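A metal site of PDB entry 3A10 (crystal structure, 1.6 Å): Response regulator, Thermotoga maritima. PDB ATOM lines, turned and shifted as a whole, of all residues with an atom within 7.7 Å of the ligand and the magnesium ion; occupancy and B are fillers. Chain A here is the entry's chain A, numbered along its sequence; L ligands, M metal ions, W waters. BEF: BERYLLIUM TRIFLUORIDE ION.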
ATOM      1  N   VAL A   7      -8.300  -3.450 -31.615  1.00  0.00           N
ATOM      2  CA  VAL A   7      -8.688  -4.756 -32.135  1.00  0.00           C
ATOM      3  C   VAL A   7     -10.155  -5.005 -31.820  1.00  0.00           C
ATOM      4  O   VAL A   7     -10.529  -5.064 -30.662  1.00  0.00           O
ATOM      5  CB  VAL A   7      -7.838  -5.881 -31.501  1.00  0.00           C
ATOM      6  CG1 VAL A   7      -8.111  -7.218 -32.185  1.00  0.00           C
ATOM      7  CG2 VAL A   7      -6.318  -5.528 -31.607  1.00  0.00           C
ATOM      8  N   ASP A   8     -10.975  -5.124 -32.866  1.00  0.00           N
ATOM      9  CA  ASP A   8     -12.388  -5.432 -32.662  1.00  0.00           C
ATOM     10  C   ASP A   8     -12.941  -6.037 -33.954  1.00  0.00           C
ATOM     11  O   ASP A   8     -12.558  -5.595 -35.040  1.00  0.00           O
ATOM     12  CB  ASP A   8     -13.152  -4.170 -32.263  1.00  0.00           C
ATOM     13  CG  ASP A   8     -14.531  -4.473 -31.700  1.00  0.00           C
ATOM     14  OD1 ASP A   8     -15.385  -4.996 -32.428  1.00  0.00           O
ATOM     15  OD2 ASP A   8     -14.768  -4.126 -30.546  1.00  0.00           O
ATOM     16  N   ASP A   9     -13.827  -7.023 -33.832  1.00  0.00           N
ATOM     17  CA  ASP A   9     -14.347  -7.704 -35.027  1.00  0.00           C
ATOM     18  C   ASP A   9     -15.409  -6.898 -35.752  1.00  0.00           C
ATOM     19  O   ASP A   9     -15.718  -7.173 -36.912  1.00  0.00           O
ATOM     20  CB  ASP A   9     -14.895  -9.095 -34.704  1.00  0.00           C
ATOM     21  CG  ASP A   9     -16.033  -9.065 -33.690  1.00  0.00           C
ATOM     22  OD1 ASP A   9     -15.875  -8.422 -32.645  1.00  0.00           O
ATOM     23  OD2 ASP A   9     -17.061  -9.761 -33.915  1.00  0.00           O
ATOM     24  N   GLU A  10     -15.997  -5.922 -35.071  1.00  0.00           N
ATOM     25  CA  GLU A  10     -17.052  -5.139 -35.680  1.00  0.00           C
ATOM     26  C   GLU A  10     -16.507  -3.896 -36.376  1.00  0.00           C
ATOM     27  O   GLU A  10     -16.021  -2.969 -35.701  1.00  0.00           O
ATOM     28  CB  GLU A  10     -18.116  -4.787 -34.645  1.00  0.00           C
ATOM     29  CG  GLU A  10     -18.792  -6.016 -34.085  1.00  0.00           C
ATOM     30  CD  GLU A  10     -19.860  -5.683 -33.090  1.00  0.00           C
ATOM     31  OE1 GLU A  10     -20.961  -5.291 -33.526  1.00  0.00           O
ATOM     32  OE2 GLU A  10     -19.603  -5.808 -31.881  1.00  0.00           O
ATOM     33  N   ILE A  13     -17.553  -0.394 -35.127  1.00  0.00           N
ATOM     34  CA  ILE A  13     -16.997  -0.123 -33.798  1.00  0.00           C
ATOM     35  C   ILE A  13     -15.522   0.214 -33.887  1.00  0.00           C
ATOM     36  O   ILE A  13     -15.061   1.175 -33.227  1.00  0.00           O
ATOM     37  CB  ILE A  13     -17.242  -1.327 -32.794  1.00  0.00           C
ATOM     38  CG1 ILE A  13     -18.750  -1.629 -32.674  1.00  0.00           C
ATOM     39  CG2 ILE A  13     -16.591  -1.045 -31.423  1.00  0.00           C
ATOM     40  CD1 ILE A  13     -19.629  -0.476 -32.262  1.00  0.00           C
ATOM     41  N   GLU A  32      -8.868  -6.779 -37.241  1.00  0.00           N
ATOM     42  CA  GLU A  32     -10.240  -7.272 -37.284  1.00  0.00           C
ATOM     43  C   GLU A  32     -10.421  -8.617 -36.592  1.00  0.00           C
ATOM     44  O   GLU A  32     -11.554  -9.077 -36.434  1.00  0.00           O
ATOM     45  CB  GLU A  32     -10.727  -7.363 -38.732  1.00  0.00           C
ATOM     46  CG  GLU A  32     -10.078  -8.448 -39.555  1.00  0.00           C
ATOM     47  CD  GLU A  32     -10.539  -8.436 -40.996  1.00  0.00           C
ATOM     48  OE1 GLU A  32     -11.603  -7.826 -41.286  1.00  0.00           O
ATOM     49  OE2 GLU A  32      -9.835  -9.030 -41.842  1.00  0.00           O
ATOM     50  N   LEU A  51      -8.270  -4.243 -26.748  1.00  0.00           N
ATOM     51  CA  LEU A  51      -8.656  -5.540 -27.247  1.00  0.00           C
ATOM     52  C   LEU A  51     -10.088  -5.889 -26.897  1.00  0.00           C
ATOM     53  O   LEU A  51     -10.438  -6.004 -25.733  1.00  0.00           O
ATOM     54  CB  LEU A  51      -7.777  -6.659 -26.623  1.00  0.00           C
ATOM     55  CG  LEU A  51      -6.299  -6.846 -26.973  1.00  0.00           C
ATOM     56  CD1 LEU A  51      -5.835  -7.964 -26.058  1.00  0.00           C
ATOM     57  CD2 LEU A  51      -6.089  -7.178 -28.436  1.00  0.00           C
ATOM     58  N   ASP A  52     -10.891  -6.079 -27.945  1.00  0.00           N
ATOM     59  CA  ASP A  52     -12.222  -6.698 -27.816  1.00  0.00           C
ATOM     60  C   ASP A  52     -12.057  -8.154 -27.385  1.00  0.00           C
ATOM     61  O   ASP A  52     -11.002  -8.764 -27.642  1.00  0.00           O
ATOM     62  CB  ASP A  52     -12.861  -6.675 -29.196  1.00  0.00           C
ATOM     63  CG  ASP A  52     -14.316  -7.095 -29.184  1.00  0.00           C
ATOM     64  OD1 ASP A  52     -14.993  -6.887 -28.157  1.00  0.00           O
ATOM     65  OD2 ASP A  52     -14.744  -7.609 -30.227  1.00  0.00           O
ATOM     66  N   ILE A  53     -13.071  -8.717 -26.743  1.00  0.00           N
ATOM     67  CA  ILE A  53     -12.966 -10.117 -26.284  1.00  0.00           C
ATOM     68  C   ILE A  53     -13.645 -11.034 -27.295  1.00  0.00           C
ATOM     69  O   ILE A  53     -13.015 -11.936 -27.846  1.00  0.00           O
ATOM     70  CB  ILE A  53     -13.518 -10.355 -24.844  1.00  0.00           C
ATOM     71  CG1 ILE A  53     -12.596  -9.711 -23.807  1.00  0.00           C
ATOM     72  CG2 ILE A  53     -13.704 -11.885 -24.585  1.00  0.00           C
ATOM     73  CD1 ILE A  53     -13.134  -9.657 -22.355  1.00  0.00           C
ATOM     74  N   GLU A  54     -14.931 -10.786 -27.576  1.00  0.00           N
ATOM     75  CA  GLU A  54     -15.676 -11.663 -28.471  1.00  0.00           C
ATOM     76  C   GLU A  54     -15.429 -11.388 -29.957  1.00  0.00           C
ATOM     77  O   GLU A  54     -15.828 -10.343 -30.487  1.00  0.00           O
ATOM     78  CB  GLU A  54     -17.175 -11.612 -28.129  1.00  0.00           C
ATOM     79  CG  GLU A  54     -17.460 -11.948 -26.680  1.00  0.00           C
ATOM     80  CD  GLU A  54     -18.933 -12.258 -26.444  1.00  0.00           C
ATOM     81  OE1 GLU A  54     -19.754 -11.897 -27.324  1.00  0.00           O
ATOM     82  OE2 GLU A  54     -19.243 -12.841 -25.387  1.00  0.00           O
ATOM     83  N   MET A  55     -14.750 -12.341 -30.617  1.00  0.00           N
ATOM     84  CA  MET A  55     -14.402 -12.216 -32.034  1.00  0.00           C
ATOM     85  C   MET A  55     -14.434 -13.601 -32.672  1.00  0.00           C
ATOM     86  O   MET A  55     -14.219 -14.561 -31.977  1.00  0.00           O
ATOM     87  CB  MET A  55     -12.993 -11.642 -32.188  1.00  0.00           C
ATOM     88  CG  MET A  55     -12.861 -10.241 -31.617  1.00  0.00           C
ATOM     89  SD  MET A  55     -11.133  -9.455 -31.986  1.00  0.00           S
ATOM     90  CE  MET A  55     -10.112 -10.403 -30.615  1.00  0.00           C
ATOM     91  N   PRO A  56     -14.699 -13.694 -33.984  1.00  0.00           N
ATOM     92  CA  PRO A  56     -14.547 -15.002 -34.626  1.00  0.00           C
ATOM     93  C   PRO A  56     -13.075 -15.417 -34.570  1.00  0.00           C
ATOM     94  O   PRO A  56     -12.179 -14.602 -34.834  1.00  0.00           O
ATOM     95  CB  PRO A  56     -14.967 -14.749 -36.071  1.00  0.00           C
ATOM     96  CG  PRO A  56     -15.706 -13.467 -36.063  1.00  0.00           C
ATOM     97  CD  PRO A  56     -15.103 -12.659 -34.968  1.00  0.00           C
ATOM     98  N   GLY A  60     -10.243 -12.330 -27.507  1.00  0.00           N
ATOM     99  CA  GLY A  60      -9.384 -11.298 -26.976  1.00  0.00           C
ATOM    100  C   GLY A  60      -8.659 -11.673 -25.692  1.00  0.00           C
ATOM    101  O   GLY A  60      -7.603 -11.131 -25.405  1.00  0.00           O
ATOM    102  N   LEU A  79     -11.432  -4.053 -23.883  1.00  0.00           N
ATOM    103  CA  LEU A  79     -12.584  -3.188 -24.135  1.00  0.00           C
ATOM    104  C   LEU A  79     -13.669  -4.017 -24.790  1.00  0.00           C
ATOM    105  O   LEU A  79     -13.582  -4.360 -25.977  1.00  0.00           O
ATOM    106  CB  LEU A  79     -12.190  -2.003 -24.999  1.00  0.00           C
ATOM    107  CG  LEU A  79     -13.349  -1.094 -25.431  1.00  0.00           C
ATOM    108  CD1 LEU A  79     -14.002  -0.395 -24.216  1.00  0.00           C
ATOM    109  CD2 LEU A  79     -12.866  -0.085 -26.495  1.00  0.00           C
ATOM    110  N   THR A  80     -14.697  -4.343 -24.007  1.00  0.00           N
ATOM    111  CA  THR A  80     -15.684  -5.324 -24.412  1.00  0.00           C
ATOM    112  C   THR A  80     -17.079  -4.806 -24.066  1.00  0.00           C
ATOM    113  O   THR A  80     -17.236  -4.022 -23.121  1.00  0.00           O
ATOM    114  CB  THR A  80     -15.439  -6.681 -23.707  1.00  0.00           C
ATOM    115  OG1 THR A  80     -16.505  -7.592 -24.014  1.00  0.00           O
ATOM    116  CG2 THR A  80     -15.267  -6.506 -22.187  1.00  0.00           C
ATOM    117  N   ALA A  81     -18.083  -5.222 -24.832  1.00  0.00           N
ATOM    118  CA  ALA A  81     -19.458  -4.874 -24.505  1.00  0.00           C
ATOM    119  C   ALA A  81     -19.897  -5.482 -23.180  1.00  0.00           C
ATOM    120  O   ALA A  81     -20.845  -4.979 -22.542  1.00  0.00           O
ATOM    121  CB  ALA A  81     -20.407  -5.307 -25.607  1.00  0.00           C
ATOM    122  N   TYR A  82     -19.220  -6.556 -22.765  1.00  0.00           N
ATOM    123  CA  TYR A  82     -19.726  -7.450 -21.709  1.00  0.00           C
ATOM    124  C   TYR A  82     -18.915  -7.423 -20.443  1.00  0.00           C
ATOM    125  O   TYR A  82     -17.700  -7.586 -20.481  1.00  0.00           O
ATOM    126  CB  TYR A  82     -19.816  -8.876 -22.272  1.00  0.00           C
ATOM    127  CG  TYR A  82     -20.608  -8.890 -23.566  1.00  0.00           C
ATOM    128  CD1 TYR A  82     -21.996  -8.678 -23.555  1.00  0.00           C
ATOM    129  CD2 TYR A  82     -19.960  -9.038 -24.807  1.00  0.00           C
ATOM    130  CE1 TYR A  82     -22.739  -8.658 -24.730  1.00  0.00           C
ATOM    131  CE2 TYR A  82     -20.682  -9.018 -25.989  1.00  0.00           C
ATOM    132  CZ  TYR A  82     -22.084  -8.828 -25.952  1.00  0.00           C
ATOM    133  OH  TYR A  82     -22.831  -8.800 -27.126  1.00  0.00           O
ATOM    134  N   TYR A  85     -16.724 -11.081 -18.382  1.00  0.00           N
ATOM    135  CA  TYR A  85     -15.353 -11.577 -18.298  1.00  0.00           C
ATOM    136  C   TYR A  85     -14.484 -10.921 -17.222  1.00  0.00           C
ATOM    137  O   TYR A  85     -13.328 -11.344 -17.015  1.00  0.00           O
ATOM    138  CB  TYR A  85     -14.705 -11.456 -19.670  1.00  0.00           C
ATOM    139  CG  TYR A  85     -15.447 -12.120 -20.778  1.00  0.00           C
ATOM    140  CD1 TYR A  85     -15.328 -13.501 -21.002  1.00  0.00           C
ATOM    141  CD2 TYR A  85     -16.297 -11.379 -21.625  1.00  0.00           C
ATOM    142  CE1 TYR A  85     -16.029 -14.129 -22.042  1.00  0.00           C
ATOM    143  CE2 TYR A  85     -16.994 -12.002 -22.677  1.00  0.00           C
ATOM    144  CZ  TYR A  85     -16.852 -13.399 -22.866  1.00  0.00           C
ATOM    145  OH  TYR A  85     -17.479 -14.032 -23.910  1.00  0.00           O
ATOM    146  N   TYR A  97      -9.698  -3.126 -17.582  1.00  0.00           N
ATOM    147  CA  TYR A  97     -10.865  -3.748 -18.229  1.00  0.00           C
ATOM    148  C   TYR A  97     -11.910  -2.665 -18.307  1.00  0.00           C
ATOM    149  O   TYR A  97     -12.272  -2.069 -17.293  1.00  0.00           O
ATOM    150  CB  TYR A  97     -11.344  -4.911 -17.360  1.00  0.00           C
ATOM    151  CG  TYR A  97     -12.439  -5.782 -17.913  1.00  0.00           C
ATOM    152  CD1 TYR A  97     -13.743  -5.297 -18.062  1.00  0.00           C
ATOM    153  CD2 TYR A  97     -12.199  -7.119 -18.233  1.00  0.00           C
ATOM    154  CE1 TYR A  97     -14.778  -6.141 -18.573  1.00  0.00           C
ATOM    155  CE2 TYR A  97     -13.206  -7.961 -18.733  1.00  0.00           C
ATOM    156  CZ  TYR A  97     -14.510  -7.464 -18.894  1.00  0.00           C
ATOM    157  OH  TYR A  97     -15.503  -8.313 -19.367  1.00  0.00           O
ATOM    158  N   VAL A  98     -12.397  -2.399 -19.519  1.00  0.00           N
ATOM    159  CA  VAL A  98     -13.369  -1.330 -19.717  1.00  0.00           C
ATOM    160  C   VAL A  98     -14.572  -1.903 -20.449  1.00  0.00           C
ATOM    161  O   VAL A  98     -14.432  -2.561 -21.469  1.00  0.00           O
ATOM    162  CB  VAL A  98     -12.731  -0.138 -20.505  1.00  0.00           C
ATOM    163  CG1 VAL A  98     -13.746   0.941 -20.773  1.00  0.00           C
ATOM    164  CG2 VAL A  98     -11.547   0.419 -19.723  1.00  0.00           C
ATOM    165  N   LYS A 100     -17.608  -1.251 -22.850  1.00  0.00           N
ATOM    166  CA  LYS A 100     -17.944  -0.254 -23.876  1.00  0.00           C
ATOM    167  C   LYS A 100     -19.136   0.601 -23.436  1.00  0.00           C
ATOM    168  O   LYS A 100     -20.181   0.105 -22.999  1.00  0.00           O
ATOM    169  CB  LYS A 100     -18.281  -0.947 -25.185  1.00  0.00           C
ATOM    170  CG  LYS A 100     -17.109  -1.648 -25.827  1.00  0.00           C
ATOM    171  CD  LYS A 100     -17.598  -2.419 -27.080  1.00  0.00           C
ATOM    172  CE  LYS A 100     -16.465  -3.077 -27.858  1.00  0.00           C
ATOM    173  NZ  LYS A 100     -16.919  -4.155 -28.812  1.00  0.00           N
HETATM  174 BE   BEF L   1     -16.351  -7.507 -27.712  1.00  0.00          BE
HETATM  175  F1  BEF L   1     -16.104  -8.544 -26.399  1.00  0.00           F
HETATM  176  F2  BEF L   1     -17.456  -6.328 -27.213  1.00  0.00           F
HETATM  177  F3  BEF L   1     -17.135  -8.374 -28.923  1.00  0.00           F
HETATM  178 MG    MG M   1     -16.556  -8.418 -30.707  1.00  0.00          MG
HETATM  179  O   HOH W   1     -19.822  -7.129 -28.869  1.00  0.00           O
HETATM  180  O   HOH W   2     -17.161  -6.479 -30.969  1.00  0.00           O
HETATM  181  O   HOH W   3     -18.430  -9.182 -31.348  1.00  0.00           O
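A beryllium atom (BE) of the ligand is bound by the side-chain carboxylate of Asp 52, at 1.6 Å. A fluorine (F2) of the ligand is in hydrogen-bond range of the backbone NH of Ala 81 (2.7 Å). A fluorine (F1) of the ligand sits at hydrogen-bond distance from the side-chain hydroxyl (OG1) of Thr 80 (2.6 Å). F1 of the ligand lies within hydrogen-bond range of N of Ile 53, at 3.1 Å. The side-chain amino group of Lys 100 is in hydrogen-bond range of a fluorine (F2) of the ligand. The backbone NH (N) of Glu 54 is in hydrogen-bond range of a fluorine (F1) of the ligand (2.8 Å).
F3 of the ligand is bound to the magnesium ion (1.9 Å). The magnesium ion is bound by OD2 of Asp 52 (2.0 Å). Water W2 is bound to the magnesium ion (2.0 Å). The magnesium ion is bound by OD1 of Asp 9 (2.1 Å). The magnesium ion is bound by O of Glu 54, at 2.1 Å. The magnesium ion is bound by water W3. The magnesium ion has six donor atoms within binding distance.
Water W2 lies within hydrogen-bond range of OE2 of Glu 10 (2.7 Å), OD1 of Asp 8 (2.7 Å) and NZ of Lys 100 (3.2 Å). Water W1 lies within hydrogen-bond range of F2 of the ligand and OE2 of Glu 10.
Of the 21 residues printed, 7 come within 4 Å of the ligand.
Three residues have an atom within 4 Å of the magnesium ion: Asp 9, Asp 52 and Glu 54. The nearest printed residue that does not touch the magnesium ion is Asp 8 (4.01 Å).
O of Val 98 sits at hydrogen-bond distance from N of Thr 80, at 3.1 Å. The backbone NH of Asp 52 is in hydrogen-bond range of the backbone carbonyl oxygen of Val 7 (2.9 Å). O of Thr 80 is in hydrogen-bond range of N of Lys 100, at 2.8 Å. The side-chain hydroxyl (OG1) of Thr 80 lies close to the backbone NH (N) of Tyr 82, at 3.2 Å. The side-chain carboxylate of Asp 8 is in salt-bridge range of the side-chain amino group of Lys 100 (2.8 Å). OD1 of Asp 52 lies close to NZ of Lys 100, at 3.4 Å. The backbone NH (N) of Gly 60 lies within hydrogen-bond range of the backbone carbonyl oxygen (O) of Ile 53 (2.8 Å). OH of Tyr 85 lies within hydrogen-bond range of OE2 of Glu 54 (2.6 Å).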
